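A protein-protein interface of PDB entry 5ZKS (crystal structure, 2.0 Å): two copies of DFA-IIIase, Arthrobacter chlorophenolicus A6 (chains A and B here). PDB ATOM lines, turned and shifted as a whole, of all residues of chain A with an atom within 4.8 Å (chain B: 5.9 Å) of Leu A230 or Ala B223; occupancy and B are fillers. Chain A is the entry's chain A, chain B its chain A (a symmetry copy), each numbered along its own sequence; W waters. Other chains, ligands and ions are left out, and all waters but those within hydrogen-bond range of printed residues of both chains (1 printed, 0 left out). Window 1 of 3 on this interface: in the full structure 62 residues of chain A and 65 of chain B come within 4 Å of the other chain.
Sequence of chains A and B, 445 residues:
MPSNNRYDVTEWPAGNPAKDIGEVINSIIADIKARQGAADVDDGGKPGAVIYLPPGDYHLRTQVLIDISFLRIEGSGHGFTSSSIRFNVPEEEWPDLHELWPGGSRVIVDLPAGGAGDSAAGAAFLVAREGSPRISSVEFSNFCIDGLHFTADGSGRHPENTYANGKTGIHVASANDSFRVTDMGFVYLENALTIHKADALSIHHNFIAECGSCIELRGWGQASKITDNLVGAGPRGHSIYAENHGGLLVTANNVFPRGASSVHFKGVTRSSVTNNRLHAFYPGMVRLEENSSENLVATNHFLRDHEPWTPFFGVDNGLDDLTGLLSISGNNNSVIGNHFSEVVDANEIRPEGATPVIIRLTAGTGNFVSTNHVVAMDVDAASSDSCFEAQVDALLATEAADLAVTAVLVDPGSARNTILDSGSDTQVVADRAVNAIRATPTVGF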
ATOM      1  N   ASN A 206     -24.689   8.774 -11.343  1.00  0.00           N
ATOM      2  CA  ASN A 206     -24.377  10.163 -11.554  1.00  0.00           C
ATOM      3  C   ASN A 206     -23.401  10.642 -10.484  1.00  0.00           C
ATOM      4  O   ASN A 206     -23.137   9.956  -9.482  1.00  0.00           O
ATOM      5  CB  ASN A 206     -25.664  11.009 -11.559  1.00  0.00           C
ATOM      6  CG  ASN A 206     -26.665  10.515 -12.578  1.00  0.00           C
ATOM      7  OD1 ASN A 206     -26.570  10.807 -13.766  1.00  0.00           O
ATOM      8  ND2 ASN A 206     -27.603   9.727 -12.121  1.00  0.00           N
ATOM      9  N   PHE A 207     -22.823  11.802 -10.753  1.00  0.00           N
ATOM     10  CA  PHE A 207     -22.039  12.547  -9.782  1.00  0.00           C
ATOM     11  C   PHE A 207     -22.773  13.864  -9.536  1.00  0.00           C
ATOM     12  O   PHE A 207     -22.832  14.704 -10.424  1.00  0.00           O
ATOM     13  CB  PHE A 207     -20.654  12.827 -10.344  1.00  0.00           C
ATOM     14  CG  PHE A 207     -19.622  13.094  -9.291  1.00  0.00           C
ATOM     15  CD1 PHE A 207     -19.439  14.374  -8.791  1.00  0.00           C
ATOM     16  CD2 PHE A 207     -18.818  12.067  -8.820  1.00  0.00           C
ATOM     17  CE1 PHE A 207     -18.485  14.625  -7.828  1.00  0.00           C
ATOM     18  CE2 PHE A 207     -17.860  12.306  -7.848  1.00  0.00           C
ATOM     19  CZ  PHE A 207     -17.694  13.594  -7.351  1.00  0.00           C
ATOM     20  N   ILE A 208     -23.306  14.041  -8.331  1.00  0.00           N
ATOM     21  CA  ILE A 208     -24.216  15.138  -8.023  1.00  0.00           C
ATOM     22  C   ILE A 208     -23.679  15.742  -6.735  1.00  0.00           C
ATOM     23  O   ILE A 208     -23.957  15.254  -5.651  1.00  0.00           O
ATOM     24  CB  ILE A 208     -25.677  14.637  -7.853  1.00  0.00           C
ATOM     25  CG1 ILE A 208     -25.994  13.546  -8.886  1.00  0.00           C
ATOM     26  CG2 ILE A 208     -26.661  15.791  -7.975  1.00  0.00           C
ATOM     27  CD1 ILE A 208     -27.441  13.110  -8.925  1.00  0.00           C
ATOM     28  N   ASP A 228     -26.209   3.797  -7.349  1.00  0.00           N
ATOM     29  CA  ASP A 228     -24.814   3.969  -7.785  1.00  0.00           C
ATOM     30  C   ASP A 228     -24.411   5.417  -8.000  1.00  0.00           C
ATOM     31  O   ASP A 228     -23.520   5.699  -8.779  1.00  0.00           O
ATOM     32  CB  ASP A 228     -24.518   3.138  -9.032  1.00  0.00           C
ATOM     33  CG  ASP A 228     -23.524   2.039  -8.759  1.00  0.00           C
ATOM     34  OD1 ASP A 228     -22.337   2.343  -8.498  1.00  0.00           O
ATOM     35  OD2 ASP A 228     -23.939   0.873  -8.780  1.00  0.00           O
ATOM     36  N   ASN A 229     -25.047   6.327  -7.270  1.00  0.00           N
ATOM     37  CA  ASN A 229     -24.694   7.727  -7.371  1.00  0.00           C
ATOM     38  C   ASN A 229     -23.661   8.128  -6.324  1.00  0.00           C
ATOM     39  O   ASN A 229     -23.587   7.569  -5.216  1.00  0.00           O
ATOM     40  CB  ASN A 229     -25.942   8.611  -7.235  1.00  0.00           C
ATOM     41  CG  ASN A 229     -26.993   8.296  -8.288  1.00  0.00           C
ATOM     42  OD1 ASN A 229     -26.871   8.697  -9.442  1.00  0.00           O
ATOM     43  ND2 ASN A 229     -28.040   7.602  -7.891  1.00  0.00           N
ATOM     44  N   LEU A 230     -22.837   9.087  -6.712  1.00  0.00           N
ATOM     45  CA  LEU A 230     -22.057   9.843  -5.776  1.00  0.00           C
ATOM     46  C   LEU A 230     -22.752  11.182  -5.541  1.00  0.00           C
ATOM     47  O   LEU A 230     -22.965  11.938  -6.484  1.00  0.00           O
ATOM     48  CB  LEU A 230     -20.672  10.046  -6.350  1.00  0.00           C
ATOM     49  CG  LEU A 230     -19.825   8.771  -6.279  1.00  0.00           C
ATOM     50  CD1 LEU A 230     -18.727   8.753  -7.322  1.00  0.00           C
ATOM     51  CD2 LEU A 230     -19.212   8.604  -4.904  1.00  0.00           C
ATOM     52  N   VAL A 231     -23.057  11.492  -4.280  1.00  0.00           N
ATOM     53  CA  VAL A 231     -23.961  12.593  -3.941  1.00  0.00           C
ATOM     54  C   VAL A 231     -23.445  13.384  -2.752  1.00  0.00           C
ATOM     55  O   VAL A 231     -23.156  12.803  -1.714  1.00  0.00           O
ATOM     56  CB  VAL A 231     -25.362  12.061  -3.571  1.00  0.00           C
ATOM     57  CG1 VAL A 231     -26.360  13.198  -3.347  1.00  0.00           C
ATOM     58  CG2 VAL A 231     -25.875  11.121  -4.652  1.00  0.00           C
ATOM     59  N   GLY A 232     -23.367  14.707  -2.914  1.00  0.00           N
ATOM     60  CA  GLY A 232     -22.997  15.637  -1.841  1.00  0.00           C
ATOM     61  C   GLY A 232     -23.795  16.929  -1.943  1.00  0.00           C
ATOM     62  O   GLY A 232     -23.715  17.636  -2.941  1.00  0.00           O
ATOM     63  N   ASN A 254     -23.122   6.343  -2.694  1.00  0.00           N
ATOM     64  CA  ASN A 254     -22.132   6.827  -1.758  1.00  0.00           C
ATOM     65  C   ASN A 254     -22.435   8.292  -1.531  1.00  0.00           C
ATOM     66  O   ASN A 254     -22.156   9.126  -2.370  1.00  0.00           O
ATOM     67  CB  ASN A 254     -20.728   6.612  -2.296  1.00  0.00           C
ATOM     68  CG  ASN A 254     -19.683   6.852  -1.251  1.00  0.00           C
ATOM     69  OD1 ASN A 254     -19.784   7.819  -0.504  1.00  0.00           O
ATOM     70  ND2 ASN A 254     -18.691   5.974  -1.169  1.00  0.00           N
ATOM     71  N   PHE A 256     -22.006  11.645   0.528  1.00  0.00           N
ATOM     72  CA  PHE A 256     -21.058  12.285   1.470  1.00  0.00           C
ATOM     73  C   PHE A 256     -21.570  13.667   1.874  1.00  0.00           C
ATOM     74  O   PHE A 256     -22.521  14.127   1.321  1.00  0.00           O
ATOM     75  CB  PHE A 256     -19.661  12.292   0.862  1.00  0.00           C
ATOM     76  CG  PHE A 256     -19.649  12.686  -0.586  1.00  0.00           C
ATOM     77  CD1 PHE A 256     -19.670  14.015  -0.949  1.00  0.00           C
ATOM     78  CD2 PHE A 256     -19.653  11.733  -1.583  1.00  0.00           C
ATOM     79  CE1 PHE A 256     -19.673  14.373  -2.283  1.00  0.00           C
ATOM     80  CE2 PHE A 256     -19.657  12.094  -2.913  1.00  0.00           C
ATOM     81  CZ  PHE A 256     -19.663  13.416  -3.257  1.00  0.00           C
ATOM     82  N   ARG A 277     -23.597   3.796   1.415  1.00  0.00           N
ATOM     83  CA  ARG A 277     -22.596   4.340   2.302  1.00  0.00           C
ATOM     84  C   ARG A 277     -23.006   5.790   2.505  1.00  0.00           C
ATOM     85  O   ARG A 277     -23.171   6.533   1.538  1.00  0.00           O
ATOM     86  CB  ARG A 277     -21.198   4.216   1.700  1.00  0.00           C
ATOM     87  CG  ARG A 277     -20.099   4.718   2.636  1.00  0.00           C
ATOM     88  CD  ARG A 277     -19.825   6.191   2.360  1.00  0.00           C
ATOM     89  NE  ARG A 277     -18.917   6.803   3.322  1.00  0.00           N
ATOM     90  CZ  ARG A 277     -18.222   7.926   3.108  1.00  0.00           C
ATOM     91  NH1 ARG A 277     -18.283   8.570   1.944  1.00  0.00           N
ATOM     92  NH2 ARG A 277     -17.420   8.388   4.058  1.00  0.00           N
ATOM     93  N   ALA B 198      -7.125   8.262  -4.590  1.00  0.00           N
ATOM     94  CA  ALA B 198      -8.434   8.475  -5.230  1.00  0.00           C
ATOM     95  C   ALA B 198      -9.478   9.094  -4.305  1.00  0.00           C
ATOM     96  O   ALA B 198      -9.668   8.635  -3.173  1.00  0.00           O
ATOM     97  CB  ALA B 198      -8.962   7.155  -5.768  1.00  0.00           C
ATOM     98  N   ASP B 199     -10.146  10.134  -4.798  1.00  0.00           N
ATOM     99  CA  ASP B 199     -11.301  10.723  -4.139  1.00  0.00           C
ATOM    100  C   ASP B 199     -12.545  10.554  -5.028  1.00  0.00           C
ATOM    101  O   ASP B 199     -12.543  10.924  -6.191  1.00  0.00           O
ATOM    102  CB  ASP B 199     -11.059  12.212  -3.896  1.00  0.00           C
ATOM    103  CG  ASP B 199     -12.089  12.844  -2.954  1.00  0.00           C
ATOM    104  OD1 ASP B 199     -13.150  12.243  -2.684  1.00  0.00           O
ATOM    105  OD2 ASP B 199     -11.833  13.975  -2.473  1.00  0.00           O
ATOM    106  N   ALA B 200     -13.606   9.990  -4.476  1.00  0.00           N
ATOM    107  CA  ALA B 200     -14.897   9.953  -5.187  1.00  0.00           C
ATOM    108  C   ALA B 200     -14.772   9.309  -6.566  1.00  0.00           C
ATOM    109  O   ALA B 200     -15.367   9.752  -7.556  1.00  0.00           O
ATOM    110  CB  ALA B 200     -15.489  11.351  -5.287  1.00  0.00           C
ATOM    111  N   LEU B 201     -13.987   8.243  -6.596  1.00  0.00           N
ATOM    112  CA  LEU B 201     -13.816   7.417  -7.772  1.00  0.00           C
ATOM    113  C   LEU B 201     -14.973   6.405  -7.941  1.00  0.00           C
ATOM    114  O   LEU B 201     -15.497   5.860  -6.964  1.00  0.00           O
ATOM    115  CB  LEU B 201     -12.470   6.674  -7.647  1.00  0.00           C
ATOM    116  CG  LEU B 201     -12.211   5.413  -8.469  1.00  0.00           C
ATOM    117  CD1 LEU B 201     -11.798   5.779  -9.883  1.00  0.00           C
ATOM    118  CD2 LEU B 201     -11.120   4.603  -7.802  1.00  0.00           C
ATOM    119  N   SER B 202     -15.351   6.143  -9.189  1.00  0.00           N
ATOM    120  CA  SER B 202     -16.282   5.059  -9.513  1.00  0.00           C
ATOM    121  C   SER B 202     -15.670   4.075 -10.514  1.00  0.00           C
ATOM    122  O   SER B 202     -15.363   4.423 -11.657  1.00  0.00           O
ATOM    123  CB  SER B 202     -17.589   5.613 -10.055  1.00  0.00           C
ATOM    124  OG  SER B 202     -18.526   4.559 -10.204  1.00  0.00           O
ATOM    125  N   GLY B 221      -7.289   7.074   0.129  1.00  0.00           N
ATOM    126  CA  GLY B 221      -8.426   7.565  -0.608  1.00  0.00           C
ATOM    127  C   GLY B 221      -9.662   7.730   0.210  1.00  0.00           C
ATOM    128  O   GLY B 221      -9.689   7.442   1.406  1.00  0.00           O
ATOM    129  N   GLN B 222     -10.707   8.183  -0.462  1.00  0.00           N
ATOM    130  CA  GLN B 222     -11.957   8.383   0.199  1.00  0.00           C
ATOM    131  C   GLN B 222     -13.166   8.444  -0.733  1.00  0.00           C
ATOM    132  O   GLN B 222     -13.065   8.755  -1.928  1.00  0.00           O
ATOM    133  CB  GLN B 222     -11.904   9.660   1.035  1.00  0.00           C
ATOM    134  CG  GLN B 222     -11.769  10.926   0.227  1.00  0.00           C
ATOM    135  CD  GLN B 222     -11.968  12.189   1.066  1.00  0.00           C
ATOM    136  OE1 GLN B 222     -12.259  12.134   2.278  1.00  0.00           O
ATOM    137  NE2 GLN B 222     -11.821  13.332   0.426  1.00  0.00           N
ATOM    138  N   ALA B 223     -14.310   8.156  -0.132  1.00  0.00           N
ATOM    139  CA  ALA B 223     -15.624   8.312  -0.750  1.00  0.00           C
ATOM    140  C   ALA B 223     -15.766   7.716  -2.157  1.00  0.00           C
ATOM    141  O   ALA B 223     -16.454   8.279  -3.019  1.00  0.00           O
ATOM    142  CB  ALA B 223     -16.021   9.786  -0.732  1.00  0.00           C
ATOM    143  N   SER B 224     -15.139   6.557  -2.367  1.00  0.00           N
ATOM    144  CA  SER B 224     -15.144   5.888  -3.652  1.00  0.00           C
ATOM    145  C   SER B 224     -16.034   4.638  -3.670  1.00  0.00           C
ATOM    146  O   SER B 224     -16.571   4.195  -2.642  1.00  0.00           O
ATOM    147  CB  SER B 224     -13.707   5.536  -4.073  1.00  0.00           C
ATOM    148  OG  SER B 224     -12.894   6.706  -4.142  1.00  0.00           O
ATOM    149  N   LYS B 225     -16.198   4.088  -4.868  1.00  0.00           N
ATOM    150  CA  LYS B 225     -17.014   2.914  -5.043  1.00  0.00           C
ATOM    151  C   LYS B 225     -16.569   2.008  -6.177  1.00  0.00           C
ATOM    152  O   LYS B 225     -16.108   2.438  -7.258  1.00  0.00           O
ATOM    153  CB  LYS B 225     -18.485   3.303  -5.189  1.00  0.00           C
ATOM    154  CG  LYS B 225     -18.833   4.130  -6.384  1.00  0.00           C
ATOM    155  CD  LYS B 225     -20.279   4.603  -6.239  1.00  0.00           C
ATOM    156  CE  LYS B 225     -20.689   5.440  -7.428  1.00  0.00           C
ATOM    157  NZ  LYS B 225     -21.189   4.603  -8.544  1.00  0.00           N
ATOM    158  N   HIS B 245      -8.062   3.701   2.710  1.00  0.00           N
ATOM    159  CA  HIS B 245      -9.291   4.320   2.233  1.00  0.00           C
ATOM    160  C   HIS B 245     -10.251   4.479   3.376  1.00  0.00           C
ATOM    161  O   HIS B 245     -10.285   3.641   4.278  1.00  0.00           O
ATOM    162  CB  HIS B 245      -9.956   3.480   1.137  1.00  0.00           C
ATOM    163  CG  HIS B 245      -9.613   3.921  -0.243  1.00  0.00           C
ATOM    164  ND1 HIS B 245     -10.530   4.508  -1.082  1.00  0.00           N
ATOM    165  CD2 HIS B 245      -8.443   3.890  -0.925  1.00  0.00           C
ATOM    166  CE1 HIS B 245      -9.948   4.810  -2.228  1.00  0.00           C
ATOM    167  NE2 HIS B 245      -8.679   4.445  -2.158  1.00  0.00           N
ATOM    168  N   GLY B 246     -11.016   5.574   3.339  1.00  0.00           N
ATOM    169  CA  GLY B 246     -12.185   5.739   4.185  1.00  0.00           C
ATOM    170  C   GLY B 246     -13.434   5.887   3.326  1.00  0.00           C
ATOM    171  O   GLY B 246     -13.383   6.474   2.268  1.00  0.00           O
ATOM    172  N   GLY B 247     -14.561   5.345   3.764  1.00  0.00           N
ATOM    173  CA  GLY B 247     -15.821   5.548   3.039  1.00  0.00           C
ATOM    174  C   GLY B 247     -15.923   4.890   1.673  1.00  0.00           C
ATOM    175  O   GLY B 247     -16.603   5.397   0.791  1.00  0.00           O
ATOM    176  N   LEU B 248     -15.244   3.763   1.502  1.00  0.00           N
ATOM    177  CA  LEU B 248     -15.285   2.975   0.268  1.00  0.00           C
ATOM    178  C   LEU B 248     -16.505   2.055   0.318  1.00  0.00           C
ATOM    179  O   LEU B 248     -16.825   1.466   1.366  1.00  0.00           O
ATOM    180  CB  LEU B 248     -13.996   2.125   0.134  1.00  0.00           C
ATOM    181  CG  LEU B 248     -13.813   1.179  -1.067  1.00  0.00           C
ATOM    182  CD1 LEU B 248     -13.796   1.943  -2.382  1.00  0.00           C
ATOM    183  CD2 LEU B 248     -12.542   0.341  -0.944  1.00  0.00           C
HETATM  184  O   HOH W   1     -21.313   7.728  -9.998  1.00  0.00           O
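The backbone NH (N) of Ile A208 sits at hydrogen-bond distance from the backbone carbonyl oxygen (O) of Leu A230, at 2.8 Å.
The backbone NH of Asn A254 is in hydrogen-bond range of the backbone carbonyl oxygen of Asn A229 (2.8 Å).
N of Val A231 sits at hydrogen-bond distance from O of Asn A254.
OG of Ser B224 lies within hydrogen-bond range of N of Ala B200, 3.4 Å away.
OG of Ser B224 is in hydrogen-bond range of N of Leu B201 (3.1 Å).
The backbone NH of Ala B223 sits at hydrogen-bond distance from the backbone carbonyl oxygen of Gly B246 (3.1 Å).
Hydrophobic or aromatic side chains of chain B within 4 Å of the printed part of chain A: Ala B200 and Ala B223.
Of the 11 printed residues of chain A, 5 touch a printed residue of chain B.
Printed residues of chain A that touch a printed residue of chain B: Phe A207, Asp A228, Leu A230, Asn A254 and Arg A277.
Along chain A the printed residues that touch a printed residue of chain B span positions 207 to 277.
Among the printed residues, 10 pairs touch across the chains.
Leu A230 touches three residues of chain B.
Of the printed residues of chain A, Ala B200 touches Phe A207 and Leu A230.
Gln B222 touches none of the printed residues of chain A.
Ala B223 touches just these residues of chain A: Leu A230, Asn A254 and Arg A277.
Printed residues of chain A within 4 Å of Ser B224: Asn A254.
Gly B246 touches none of the printed residues of chain A.
The nearest residue of chain B that does not touch Leu A230 is Ser B202 (4.3 Å).
The nearest residue of chain A that does not touch Ala B223 is Phe A256 (4.2 Å).
Water W1 lies within hydrogen-bond range of O of Asn A206, O of Asp A228 and NZ of Lys B225.
No position is printed for both chains.
Of the 10 pairs that touch across the chains among the printed residues, none has its exchanged pair printed and touching as well.
Among the printed residues, pairs that only touch across the chains: Arg A277 with Gly B247, Leu A230 with Ala B223, Leu A230 with Ala B200, Asn A254 with Ala B223, Phe A207 with Ala B200, Leu A230 with Lys B225 and Arg A277 with Ala B223.
OD1 of Asp A228 is in salt-bridge range of NZ of Lys B225.
ND2 of Asn A254 lies within hydrogen-bond range of O of Ser B224 (3.1 Å).
ND2 of Asn A254 lies within hydrogen-bond range of O of Gly B247, 2.9 Å away.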
